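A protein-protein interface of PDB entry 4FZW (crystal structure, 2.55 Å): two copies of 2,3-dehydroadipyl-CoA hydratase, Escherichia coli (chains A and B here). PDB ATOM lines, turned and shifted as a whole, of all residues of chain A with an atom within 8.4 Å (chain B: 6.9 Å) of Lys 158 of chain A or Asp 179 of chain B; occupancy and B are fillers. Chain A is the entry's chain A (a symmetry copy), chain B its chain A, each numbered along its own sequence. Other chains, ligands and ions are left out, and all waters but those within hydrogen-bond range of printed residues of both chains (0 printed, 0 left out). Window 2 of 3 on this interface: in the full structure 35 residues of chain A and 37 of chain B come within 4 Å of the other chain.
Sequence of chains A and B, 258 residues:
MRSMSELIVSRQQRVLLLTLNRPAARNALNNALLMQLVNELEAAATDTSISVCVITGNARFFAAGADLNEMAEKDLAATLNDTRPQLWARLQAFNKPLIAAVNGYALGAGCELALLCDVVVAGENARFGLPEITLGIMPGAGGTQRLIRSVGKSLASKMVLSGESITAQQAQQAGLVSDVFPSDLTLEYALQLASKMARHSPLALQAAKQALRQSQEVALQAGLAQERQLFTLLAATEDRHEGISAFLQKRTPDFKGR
The side-chain hydroxyl (OG) of Ser 154 of chain A sits at hydrogen-bond distance from the backbone NH (N) of Val 120 of chain B (2.6 Å).
The backbone carbonyl oxygen of Ser 178 of chain B sits at hydrogen-bond distance from the side-chain amino group of Lys 158 of chain A (3.4 Å).
OG of Ser 178 of chain B lies within hydrogen-bond range of OG of Ser 154 of chain A, 3.1 Å away.
NZ of Lys 158 of chain A is in salt-bridge range of OD2 of Asp 179 of chain B (2.8 Å).
N of Ser 178 of chain B is in hydrogen-bond range of O of Val 120 of chain B (3.0 Å).
The side-chain carboxylate (OE2) of Glu 164 of chain A is in salt-bridge range of the side-chain amino group (NZ) of Lys 158 of chain A, 3.8 Å away.
The backbone carbonyl oxygen (O) of Lys 153 of chain A sits at hydrogen-bond distance from the side-chain hydroxyl (OG) of Ser 157 of chain A (2.7 Å).
OG of Ser 162 of chain A is in hydrogen-bond range of O of Lys 158 of chain A (2.7 Å).
N of Ala 122 of chain B sits at hydrogen-bond distance from O of Asp 179 of chain B (3.0 Å).
The side-chain hydroxyl of Ser 162 of chain A sits close to the backbone NH of Glu 164 of chain A (3.4 Å).
O of Lys 153 of chain A touches O of Asp 118 of chain B (3.5 Å).
Asp 118 of chain B touches Ser 154 of chain A.
Val 119 of chain B touches Ser 154 of chain A (CA to OG, 3.3 Å).
CB of Ser 178 of chain B touches N of Leu 155 of chain A, 3.7 Å away.
O of Asp 118 of chain B touches CB of Ser 157 of chain A (3.6 Å).
Ser 157 of chain A touches Val 119 of chain B (CB to CG2, 3.9 Å).
Leu 212 of chain B touches Ser 157 of chain A (CD1 to OG, 3.9 Å).
CG1 of Val 160 of chain A touches CD1 of Leu 212 of chain B, at 3.7 Å.
Met 197 of chain B touches Leu 161 of chain A (SD to CB, 3.8 Å).
CG of Met 197 of chain B touches CB of Ser 162 of chain A (3.99 Å).
Of chain B, only Val 119, Ser 178 and Asp 179 come within 4 Å of Lys 158 of chain A.
Of the printed residues of chain B, Val 160 of chain A touches Leu 212.
Of the printed residues of chain B, Ser 162 of chain A touches Met 197 (3.99 Å).
Of the printed residues of chain A, Asp 118 of chain B touches Lys 153 (3.5 Å), Ser 154 (3.3 Å) and Ser 157 (3.6 Å).
Ala 122 of chain B touches none of the printed residues of chain A.
Of chain A, only Lys 158 comes within 4 Å of Asp 179 of chain B.
The nearest residue of chain B that does not touch Lys 158 of chain A is Leu 193 of chain B (4.2 Å).
The nearest residue of chain A that does not touch Asp 179 of chain B is Glu 164 of chain A (5.5 Å).
Along chain B the printed residues that touch a printed residue of chain A span positions 118 to 212.
Of the 20 printed residues of chain A, 8 touch a printed residue of chain B.
Hydrophobic or aromatic side chains of chain A that line the printed part of chain B: Val 160 and Leu 161.
Among the printed residues, 15 pairs touch across the chains.
No position is printed for both chains.
Of the 15 pairs that touch across the chains among the printed residues, none has its exchanged pair printed and touching as well.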
ATOM      1  N   LEU A 130      28.615 -32.116 -26.206  1.00  0.00           N
ATOM      2  CA  LEU A 130      28.658 -32.705 -24.896  1.00  0.00           C
ATOM      3  C   LEU A 130      27.586 -33.784 -24.789  1.00  0.00           C
ATOM      4  O   LEU A 130      26.448 -33.504 -24.398  1.00  0.00           O
ATOM      5  CB  LEU A 130      28.464 -31.615 -23.838  1.00  0.00           C
ATOM      6  CG  LEU A 130      29.607 -30.592 -23.810  1.00  0.00           C
ATOM      7  CD1 LEU A 130      29.173 -29.301 -23.129  1.00  0.00           C
ATOM      8  CD2 LEU A 130      30.898 -31.167 -23.190  1.00  0.00           C
ATOM      9  N   ILE A 133      25.155 -36.160 -21.077  1.00  0.00           N
ATOM     10  CA  ILE A 133      23.767 -36.354 -20.692  1.00  0.00           C
ATOM     11  C   ILE A 133      23.102 -37.625 -21.258  1.00  0.00           C
ATOM     12  O   ILE A 133      22.219 -38.171 -20.611  1.00  0.00           O
ATOM     13  CB  ILE A 133      22.916 -35.101 -21.035  1.00  0.00           C
ATOM     14  CG1 ILE A 133      21.609 -35.090 -20.225  1.00  0.00           C
ATOM     15  CG2 ILE A 133      22.686 -34.995 -22.558  1.00  0.00           C
ATOM     16  CD1 ILE A 133      21.809 -34.800 -18.769  1.00  0.00           C
ATOM     17  N   LEU A 147      31.233 -23.413 -21.584  1.00  0.00           N
ATOM     18  CA  LEU A 147      30.439 -23.268 -22.796  1.00  0.00           C
ATOM     19  C   LEU A 147      29.498 -22.077 -22.669  1.00  0.00           C
ATOM     20  O   LEU A 147      29.564 -21.138 -23.468  1.00  0.00           O
ATOM     21  CB  LEU A 147      29.659 -24.549 -23.091  1.00  0.00           C
ATOM     22  CG  LEU A 147      28.761 -24.542 -24.338  1.00  0.00           C
ATOM     23  CD1 LEU A 147      29.539 -24.137 -25.595  1.00  0.00           C
ATOM     24  CD2 LEU A 147      28.122 -25.899 -24.538  1.00  0.00           C
ATOM     25  N   VAL A 151      28.942 -18.924 -25.372  1.00  0.00           N
ATOM     26  CA  VAL A 151      27.821 -18.989 -26.338  1.00  0.00           C
ATOM     27  C   VAL A 151      26.442 -18.630 -25.771  1.00  0.00           C
ATOM     28  O   VAL A 151      25.460 -18.538 -26.507  1.00  0.00           O
ATOM     29  CB  VAL A 151      27.682 -20.370 -27.024  1.00  0.00           C
ATOM     30  CG1 VAL A 151      29.036 -20.910 -27.426  1.00  0.00           C
ATOM     31  CG2 VAL A 151      26.950 -21.339 -26.137  1.00  0.00           C
ATOM     32  N   GLY A 152      26.357 -18.447 -24.462  1.00  0.00           N
ATOM     33  CA  GLY A 152      25.103 -18.020 -23.870  1.00  0.00           C
ATOM     34  C   GLY A 152      24.202 -19.165 -23.473  1.00  0.00           C
ATOM     35  O   GLY A 152      24.431 -20.319 -23.861  1.00  0.00           O
ATOM     36  N   LYS A 153      23.155 -18.841 -22.716  1.00  0.00           N
ATOM     37  CA  LYS A 153      22.387 -19.857 -21.996  1.00  0.00           C
ATOM     38  C   LYS A 153      21.609 -20.842 -22.895  1.00  0.00           C
ATOM     39  O   LYS A 153      21.666 -22.062 -22.687  1.00  0.00           O
ATOM     40  CB  LYS A 153      21.446 -19.195 -20.987  1.00  0.00           C
ATOM     41  CG  LYS A 153      21.103 -20.087 -19.790  1.00  0.00           C
ATOM     42  CD  LYS A 153      19.622 -20.138 -19.472  1.00  0.00           C
ATOM     43  CE  LYS A 153      19.102 -18.792 -19.029  1.00  0.00           C
ATOM     44  NZ  LYS A 153      17.684 -18.858 -18.634  1.00  0.00           N
ATOM     45  N   SER A 154      20.901 -20.318 -23.893  1.00  0.00           N
ATOM     46  CA  SER A 154      20.033 -21.157 -24.733  1.00  0.00           C
ATOM     47  C   SER A 154      20.789 -22.264 -25.463  1.00  0.00           C
ATOM     48  O   SER A 154      20.449 -23.441 -25.339  1.00  0.00           O
ATOM     49  CB  SER A 154      19.259 -20.319 -25.749  1.00  0.00           C
ATOM     50  OG  SER A 154      18.087 -21.024 -26.103  1.00  0.00           O
ATOM     51  N   LEU A 155      21.814 -21.886 -26.214  1.00  0.00           N
ATOM     52  CA  LEU A 155      22.618 -22.871 -26.916  1.00  0.00           C
ATOM     53  C   LEU A 155      23.361 -23.845 -25.978  1.00  0.00           C
ATOM     54  O   LEU A 155      23.309 -25.054 -26.193  1.00  0.00           O
ATOM     55  CB  LEU A 155      23.594 -22.182 -27.875  1.00  0.00           C
ATOM     56  CG  LEU A 155      24.375 -23.129 -28.786  1.00  0.00           C
ATOM     57  CD1 LEU A 155      23.454 -24.034 -29.583  1.00  0.00           C
ATOM     58  CD2 LEU A 155      25.306 -22.338 -29.716  1.00  0.00           C
ATOM     59  N   ALA A 156      24.044 -23.323 -24.954  1.00  0.00           N
ATOM     60  CA  ALA A 156      24.787 -24.176 -24.039  1.00  0.00           C
ATOM     61  C   ALA A 156      23.850 -25.131 -23.324  1.00  0.00           C
ATOM     62  O   ALA A 156      24.210 -26.278 -23.048  1.00  0.00           O
ATOM     63  CB  ALA A 156      25.548 -23.355 -23.029  1.00  0.00           C
ATOM     64  N   SER A 157      22.642 -24.672 -23.017  1.00  0.00           N
ATOM     65  CA  SER A 157      21.697 -25.530 -22.313  1.00  0.00           C
ATOM     66  C   SER A 157      21.183 -26.648 -23.216  1.00  0.00           C
ATOM     67  O   SER A 157      21.160 -27.814 -22.825  1.00  0.00           O
ATOM     68  CB  SER A 157      20.571 -24.702 -21.696  1.00  0.00           C
ATOM     69  OG  SER A 157      21.119 -23.860 -20.701  1.00  0.00           O
ATOM     70  N   LYS A 158      20.799 -26.282 -24.436  1.00  0.00           N
ATOM     71  CA  LYS A 158      20.435 -27.253 -25.460  1.00  0.00           C
ATOM     72  C   LYS A 158      21.525 -28.295 -25.630  1.00  0.00           C
ATOM     73  O   LYS A 158      21.278 -29.494 -25.549  1.00  0.00           O
ATOM     74  CB  LYS A 158      20.246 -26.528 -26.768  1.00  0.00           C
ATOM     75  CG  LYS A 158      19.822 -27.400 -27.923  1.00  0.00           C
ATOM     76  CD  LYS A 158      19.785 -26.545 -29.157  1.00  0.00           C
ATOM     77  CE  LYS A 158      19.572 -27.363 -30.413  1.00  0.00           C
ATOM     78  NZ  LYS A 158      19.463 -26.441 -31.574  1.00  0.00           N
ATOM     79  N   MET A 159      22.745 -27.836 -25.854  1.00  0.00           N
ATOM     80  CA  MET A 159      23.860 -28.765 -25.991  1.00  0.00           C
ATOM     81  C   MET A 159      24.066 -29.670 -24.762  1.00  0.00           C
ATOM     82  O   MET A 159      24.262 -30.883 -24.905  1.00  0.00           O
ATOM     83  CB  MET A 159      25.148 -28.010 -26.341  1.00  0.00           C
ATOM     84  CG  MET A 159      25.200 -27.509 -27.792  1.00  0.00           C
ATOM     85  SD  MET A 159      26.654 -26.537 -28.156  1.00  0.00           S
ATOM     86  CE  MET A 159      27.908 -27.754 -27.828  1.00  0.00           C
ATOM     87  N   VAL A 160      24.021 -29.078 -23.568  1.00  0.00           N
ATOM     88  CA  VAL A 160      24.261 -29.818 -22.347  1.00  0.00           C
ATOM     89  C   VAL A 160      23.083 -30.717 -21.982  1.00  0.00           C
ATOM     90  O   VAL A 160      23.295 -31.872 -21.590  1.00  0.00           O
ATOM     91  CB  VAL A 160      24.592 -28.868 -21.181  1.00  0.00           C
ATOM     92  CG1 VAL A 160      24.360 -29.540 -19.795  1.00  0.00           C
ATOM     93  CG2 VAL A 160      26.006 -28.317 -21.337  1.00  0.00           C
ATOM     94  N   LEU A 161      21.854 -30.215 -22.138  1.00  0.00           N
ATOM     95  CA  LEU A 161      20.657 -30.992 -21.779  1.00  0.00           C
ATOM     96  C   LEU A 161      20.176 -32.040 -22.820  1.00  0.00           C
ATOM     97  O   LEU A 161      19.588 -33.068 -22.457  1.00  0.00           O
ATOM     98  CB  LEU A 161      19.500 -30.056 -21.395  1.00  0.00           C
ATOM     99  CG  LEU A 161      19.588 -29.095 -20.210  1.00  0.00           C
ATOM    100  CD1 LEU A 161      18.458 -28.077 -20.276  1.00  0.00           C
ATOM    101  CD2 LEU A 161      19.630 -29.824 -18.822  1.00  0.00           C
ATOM    102  N   SER A 162      20.434 -31.797 -24.103  1.00  0.00           N
ATOM    103  CA  SER A 162      20.079 -32.779 -25.131  1.00  0.00           C
ATOM    104  C   SER A 162      21.290 -33.571 -25.624  1.00  0.00           C
ATOM    105  O   SER A 162      21.150 -34.719 -26.026  1.00  0.00           O
ATOM    106  CB  SER A 162      19.374 -32.107 -26.307  1.00  0.00           C
ATOM    107  OG  SER A 162      20.318 -31.488 -27.159  1.00  0.00           O
ATOM    108  N   GLY A 163      22.477 -32.961 -25.586  1.00  0.00           N
ATOM    109  CA  GLY A 163      23.701 -33.627 -26.013  1.00  0.00           C
ATOM    110  C   GLY A 163      23.904 -33.672 -27.525  1.00  0.00           C
ATOM    111  O   GLY A 163      24.710 -34.472 -28.000  1.00  0.00           O
ATOM    112  N   GLU A 164      23.188 -32.831 -28.276  1.00  0.00           N
ATOM    113  CA  GLU A 164      23.378 -32.765 -29.709  1.00  0.00           C
ATOM    114  C   GLU A 164      24.570 -31.876 -30.059  1.00  0.00           C
ATOM    115  O   GLU A 164      24.810 -30.856 -29.405  1.00  0.00           O
ATOM    116  CB  GLU A 164      22.120 -32.222 -30.416  1.00  0.00           C
ATOM    117  CG  GLU A 164      21.844 -30.759 -30.103  1.00  0.00           C
ATOM    118  CD  GLU A 164      21.343 -30.004 -31.282  1.00  0.00           C
ATOM    119  OE1 GLU A 164      22.155 -29.252 -31.937  1.00  0.00           O
ATOM    120  OE2 GLU A 164      20.119 -30.155 -31.577  1.00  0.00           O
ATOM    121  N   SER A 165      25.296 -32.280 -31.102  1.00  0.00           N
ATOM    122  CA  SER A 165      26.479 -31.583 -31.602  1.00  0.00           C
ATOM    123  C   SER A 165      26.152 -30.358 -32.435  1.00  0.00           C
ATOM    124  O   SER A 165      25.029 -30.155 -32.895  1.00  0.00           O
ATOM    125  CB  SER A 165      27.302 -32.520 -32.481  1.00  0.00           C
ATOM    126  OG  SER A 165      27.814 -33.610 -31.744  1.00  0.00           O
ATOM    127  N   ILE A 166      27.169 -29.546 -32.647  1.00  0.00           N
ATOM    128  CA  ILE A 166      27.062 -28.468 -33.604  1.00  0.00           C
ATOM    129  C   ILE A 166      28.260 -28.474 -34.554  1.00  0.00           C
ATOM    130  O   ILE A 166      29.327 -29.031 -34.246  1.00  0.00           O
ATOM    131  CB  ILE A 166      26.934 -27.099 -32.911  1.00  0.00           C
ATOM    132  CG1 ILE A 166      28.089 -26.889 -31.925  1.00  0.00           C
ATOM    133  CG2 ILE A 166      25.596 -26.985 -32.194  1.00  0.00           C
ATOM    134  CD1 ILE A 166      28.243 -25.429 -31.501  1.00  0.00           C
ATOM    135  N   GLN A 170      28.410 -23.284 -36.935  1.00  0.00           N
ATOM    136  CA  GLN A 170      27.551 -22.864 -35.848  1.00  0.00           C
ATOM    137  C   GLN A 170      28.433 -22.403 -34.674  1.00  0.00           C
ATOM    138  O   GLN A 170      28.238 -21.333 -34.096  1.00  0.00           O
ATOM    139  CB  GLN A 170      26.646 -24.022 -35.449  1.00  0.00           C
ATOM    140  CG  GLN A 170      25.678 -24.406 -36.563  1.00  0.00           C
ATOM    141  CD  GLN A 170      24.848 -25.639 -36.260  1.00  0.00           C
ATOM    142  OE1 GLN A 170      25.372 -26.747 -36.141  1.00  0.00           O
ATOM    143  NE2 GLN A 170      23.543 -25.453 -36.146  1.00  0.00           N
ATOM    144  N   ASP B 118      15.447 -22.079 -20.074  1.00  0.00           N
ATOM    145  CA  ASP B 118      16.765 -22.623 -20.347  1.00  0.00           C
ATOM    146  C   ASP B 118      17.080 -22.491 -21.827  1.00  0.00           C
ATOM    147  O   ASP B 118      18.181 -22.072 -22.192  1.00  0.00           O
ATOM    148  CB  ASP B 118      16.861 -24.096 -19.897  1.00  0.00           C
ATOM    149  CG  ASP B 118      16.398 -24.303 -18.481  1.00  0.00           C
ATOM    150  OD1 ASP B 118      17.055 -23.765 -17.550  1.00  0.00           O
ATOM    151  OD2 ASP B 118      15.382 -24.999 -18.284  1.00  0.00           O
ATOM    152  N   VAL B 119      16.096 -22.816 -22.668  1.00  0.00           N
ATOM    153  CA  VAL B 119      16.299 -22.884 -24.108  1.00  0.00           C
ATOM    154  C   VAL B 119      15.168 -22.212 -24.880  1.00  0.00           C
ATOM    155  O   VAL B 119      13.995 -22.504 -24.642  1.00  0.00           O
ATOM    156  CB  VAL B 119      16.324 -24.341 -24.584  1.00  0.00           C
ATOM    157  CG1 VAL B 119      16.639 -24.408 -26.096  1.00  0.00           C
ATOM    158  CG2 VAL B 119      17.298 -25.143 -23.759  1.00  0.00           C
ATOM    159  N   VAL B 120      15.509 -21.345 -25.827  1.00  0.00           N
ATOM    160  CA  VAL B 120      14.479 -20.778 -26.686  1.00  0.00           C
ATOM    161  C   VAL B 120      14.555 -21.277 -28.141  1.00  0.00           C
ATOM    162  O   VAL B 120      15.572 -21.059 -28.829  1.00  0.00           O
ATOM    163  CB  VAL B 120      14.522 -19.237 -26.724  1.00  0.00           C
ATOM    164  CG1 VAL B 120      13.245 -18.706 -27.385  1.00  0.00           C
ATOM    165  CG2 VAL B 120      14.677 -18.664 -25.361  1.00  0.00           C
ATOM    166  N   VAL B 121      13.477 -21.922 -28.605  1.00  0.00           N
ATOM    167  CA  VAL B 121      13.262 -22.155 -30.041  1.00  0.00           C
ATOM    168  C   VAL B 121      12.238 -21.143 -30.523  1.00  0.00           C
ATOM    169  O   VAL B 121      11.145 -21.027 -29.953  1.00  0.00           O
ATOM    170  CB  VAL B 121      12.739 -23.578 -30.362  1.00  0.00           C
ATOM    171  CG1 VAL B 121      13.648 -24.666 -29.789  1.00  0.00           C
ATOM    172  CG2 VAL B 121      11.320 -23.753 -29.860  1.00  0.00           C
ATOM    173  N   ALA B 122      12.607 -20.387 -31.552  1.00  0.00           N
ATOM    174  CA  ALA B 122      11.731 -19.354 -32.084  1.00  0.00           C
ATOM    175  C   ALA B 122      11.195 -19.686 -33.500  1.00  0.00           C
ATOM    176  O   ALA B 122      11.742 -20.523 -34.223  1.00  0.00           O
ATOM    177  CB  ALA B 122      12.443 -17.995 -32.070  1.00  0.00           C
ATOM    178  N   GLY B 123      10.108 -19.029 -33.878  1.00  0.00           N
ATOM    179  CA  GLY B 123       9.609 -19.131 -35.224  1.00  0.00           C
ATOM    180  C   GLY B 123      10.184 -18.038 -36.096  1.00  0.00           C
ATOM    181  O   GLY B 123      10.611 -16.993 -35.567  1.00  0.00           O
ATOM    182  N   GLU B 124      10.170 -18.269 -37.418  1.00  0.00           N
ATOM    183  CA  GLU B 124      10.741 -17.321 -38.368  1.00  0.00           C
ATOM    184  C   GLU B 124      10.190 -15.907 -38.212  1.00  0.00           C
ATOM    185  O   GLU B 124      10.864 -14.950 -38.595  1.00  0.00           O
ATOM    186  CB  GLU B 124      10.536 -17.767 -39.823  1.00  0.00           C
ATOM    187  CG  GLU B 124      11.234 -19.034 -40.223  1.00  0.00           C
ATOM    188  CD  GLU B 124      12.731 -18.991 -40.020  1.00  0.00           C
ATOM    189  OE1 GLU B 124      13.355 -17.925 -40.228  1.00  0.00           O
ATOM    190  OE2 GLU B 124      13.287 -20.049 -39.653  1.00  0.00           O
ATOM    191  N   ALA B 168      13.694 -12.881 -35.133  1.00  0.00           N
ATOM    192  CA  ALA B 168      14.160 -14.192 -34.709  1.00  0.00           C
ATOM    193  C   ALA B 168      15.563 -14.502 -35.218  1.00  0.00           C
ATOM    194  O   ALA B 168      16.321 -15.222 -34.576  1.00  0.00           O
ATOM    195  CB  ALA B 168      13.199 -15.250 -35.185  1.00  0.00           C
ATOM    196  N   GLN B 172      18.962 -15.208 -32.967  1.00  0.00           N
ATOM    197  CA  GLN B 172      19.786 -16.428 -32.984  1.00  0.00           C
ATOM    198  C   GLN B 172      21.265 -16.123 -33.186  1.00  0.00           C
ATOM    199  O   GLN B 172      22.121 -16.828 -32.663  1.00  0.00           O
ATOM    200  CB  GLN B 172      19.338 -17.415 -34.069  1.00  0.00           C
ATOM    201  CG  GLN B 172      20.342 -18.556 -34.236  1.00  0.00           C
ATOM    202  CD  GLN B 172      19.842 -19.686 -35.095  1.00  0.00           C
ATOM    203  OE1 GLN B 172      19.020 -19.494 -36.000  1.00  0.00           O
ATOM    204  NE2 GLN B 172      20.353 -20.884 -34.833  1.00  0.00           N
ATOM    205  N   VAL B 177      18.529 -16.912 -28.791  1.00  0.00           N
ATOM    206  CA  VAL B 177      17.737 -18.048 -29.195  1.00  0.00           C
ATOM    207  C   VAL B 177      18.673 -19.048 -29.819  1.00  0.00           C
ATOM    208  O   VAL B 177      19.716 -18.681 -30.350  1.00  0.00           O
ATOM    209  CB  VAL B 177      16.630 -17.615 -30.164  1.00  0.00           C
ATOM    210  CG1 VAL B 177      16.089 -18.786 -30.905  1.00  0.00           C
ATOM    211  CG2 VAL B 177      15.526 -16.902 -29.409  1.00  0.00           C
ATOM    212  N   SER B 178      18.317 -20.319 -29.752  1.00  0.00           N
ATOM    213  CA  SER B 178      19.178 -21.332 -30.349  1.00  0.00           C
ATOM    214  C   SER B 178      18.556 -22.100 -31.542  1.00  0.00           C
ATOM    215  O   SER B 178      19.143 -23.043 -32.040  1.00  0.00           O
ATOM    216  CB  SER B 178      19.695 -22.284 -29.263  1.00  0.00           C
ATOM    217  OG  SER B 178      18.614 -22.822 -28.525  1.00  0.00           O
ATOM    218  N   ASP B 179      17.378 -21.689 -31.994  1.00  0.00           N
ATOM    219  CA  ASP B 179      16.741 -22.311 -33.153  1.00  0.00           C
ATOM    220  C   ASP B 179      15.777 -21.339 -33.810  1.00  0.00           C
ATOM    221  O   ASP B 179      15.191 -20.475 -33.156  1.00  0.00           O
ATOM    222  CB  ASP B 179      16.013 -23.608 -32.785  1.00  0.00           C
ATOM    223  CG  ASP B 179      16.865 -24.852 -33.017  1.00  0.00           C
ATOM    224  OD1 ASP B 179      17.555 -24.943 -34.055  1.00  0.00           O
ATOM    225  OD2 ASP B 179      16.853 -25.750 -32.153  1.00  0.00           O
ATOM    226  N   VAL B 180      15.668 -21.454 -35.126  1.00  0.00           N
ATOM    227  CA  VAL B 180      14.675 -20.700 -35.888  1.00  0.00           C
ATOM    228  C   VAL B 180      13.992 -21.587 -36.936  1.00  0.00           C
ATOM    229  O   VAL B 180      14.615 -22.032 -37.878  1.00  0.00           O
ATOM    230  CB  VAL B 180      15.253 -19.413 -36.526  1.00  0.00           C
ATOM    231  CG1 VAL B 180      14.158 -18.647 -37.242  1.00  0.00           C
ATOM    232  CG2 VAL B 180      15.842 -18.494 -35.456  1.00  0.00           C
ATOM    233  N   PHE B 181      12.707 -21.854 -36.731  1.00  0.00           N
ATOM    234  CA  PHE B 181      11.927 -22.743 -37.583  1.00  0.00           C
ATOM    235  C   PHE B 181      10.773 -21.998 -38.234  1.00  0.00           C
ATOM    236  O   PHE B 181      10.337 -20.970 -37.725  1.00  0.00           O
ATOM    237  CB  PHE B 181      11.345 -23.903 -36.781  1.00  0.00           C
ATOM    238  CG  PHE B 181      12.377 -24.809 -36.167  1.00  0.00           C
ATOM    239  CD1 PHE B 181      13.291 -25.493 -36.953  1.00  0.00           C
ATOM    240  CD2 PHE B 181      12.420 -24.987 -34.788  1.00  0.00           C
ATOM    241  CE1 PHE B 181      14.238 -26.331 -36.382  1.00  0.00           C
ATOM    242  CE2 PHE B 181      13.376 -25.826 -34.192  1.00  0.00           C
ATOM    243  CZ  PHE B 181      14.284 -26.498 -35.000  1.00  0.00           C
ATOM    244  N   THR B 186       7.440 -24.494 -35.306  1.00  0.00           N
ATOM    245  CA  THR B 186       8.128 -24.131 -34.076  1.00  0.00           C
ATOM    246  C   THR B 186       7.689 -25.005 -32.884  1.00  0.00           C
ATOM    247  O   THR B 186       8.504 -25.651 -32.228  1.00  0.00           O
ATOM    248  CB  THR B 186       7.869 -22.637 -33.704  1.00  0.00           C
ATOM    249  OG1 THR B 186       7.880 -21.817 -34.883  1.00  0.00           O
ATOM    250  CG2 THR B 186       8.926 -22.134 -32.699  1.00  0.00           C
ATOM    251  N   TYR B 189       8.497 -28.688 -33.329  1.00  0.00           N
ATOM    252  CA  TYR B 189       9.926 -28.932 -33.263  1.00  0.00           C
ATOM    253  C   TYR B 189      10.428 -28.720 -31.828  1.00  0.00           C
ATOM    254  O   TYR B 189      11.318 -29.432 -31.363  1.00  0.00           O
ATOM    255  CB  TYR B 189      10.671 -28.044 -34.282  1.00  0.00           C
ATOM    256  CG  TYR B 189      10.583 -28.583 -35.679  1.00  0.00           C
ATOM    257  CD1 TYR B 189       9.898 -29.768 -35.930  1.00  0.00           C
ATOM    258  CD2 TYR B 189      11.184 -27.933 -36.748  1.00  0.00           C
ATOM    259  CE1 TYR B 189       9.809 -30.296 -37.190  1.00  0.00           C
ATOM    260  CE2 TYR B 189      11.094 -28.462 -38.064  1.00  0.00           C
ATOM    261  CZ  TYR B 189      10.409 -29.645 -38.263  1.00  0.00           C
ATOM    262  OH  TYR B 189      10.308 -30.176 -39.525  1.00  0.00           O
ATOM    263  N   LEU B 193      12.392 -31.459 -29.568  1.00  0.00           N
ATOM    264  CA  LEU B 193      13.544 -31.100 -28.743  1.00  0.00           C
ATOM    265  C   LEU B 193      13.304 -31.632 -27.331  1.00  0.00           C
ATOM    266  O   LEU B 193      14.151 -32.333 -26.778  1.00  0.00           O
ATOM    267  CB  LEU B 193      13.790 -29.584 -28.707  1.00  0.00           C
ATOM    268  CG  LEU B 193      14.953 -29.138 -27.805  1.00  0.00           C
ATOM    269  CD1 LEU B 193      16.301 -29.656 -28.309  1.00  0.00           C
ATOM    270  CD2 LEU B 193      14.989 -27.620 -27.616  1.00  0.00           C
ATOM    271  N   MET B 197      15.327 -34.608 -24.789  1.00  0.00           N
ATOM    272  CA  MET B 197      15.825 -34.375 -23.450  1.00  0.00           C
ATOM    273  C   MET B 197      15.194 -35.372 -22.475  1.00  0.00           C
ATOM    274  O   MET B 197      15.893 -35.991 -21.657  1.00  0.00           O
ATOM    275  CB  MET B 197      15.549 -32.921 -23.013  1.00  0.00           C
ATOM    276  CG  MET B 197      16.179 -31.889 -23.931  1.00  0.00           C
ATOM    277  SD  MET B 197      16.168 -30.228 -23.254  1.00  0.00           S
ATOM    278  CE  MET B 197      14.560 -30.215 -22.502  1.00  0.00           C
ATOM    279  N   LEU B 212      24.134 -25.563 -14.591  1.00  0.00           N
ATOM    280  CA  LEU B 212      23.982 -24.446 -15.520  1.00  0.00           C
ATOM    281  C   LEU B 212      23.502 -23.171 -14.844  1.00  0.00           C
ATOM    282  O   LEU B 212      24.045 -22.093 -15.113  1.00  0.00           O
ATOM    283  CB  LEU B 212      23.069 -24.811 -16.705  1.00  0.00           C
ATOM    284  CG  LEU B 212      23.666 -25.708 -17.785  1.00  0.00           C
ATOM    285  CD1 LEU B 212      22.578 -26.588 -18.384  1.00  0.00           C
ATOM    286  CD2 LEU B 212      24.363 -24.867 -18.845  1.00  0.00           C
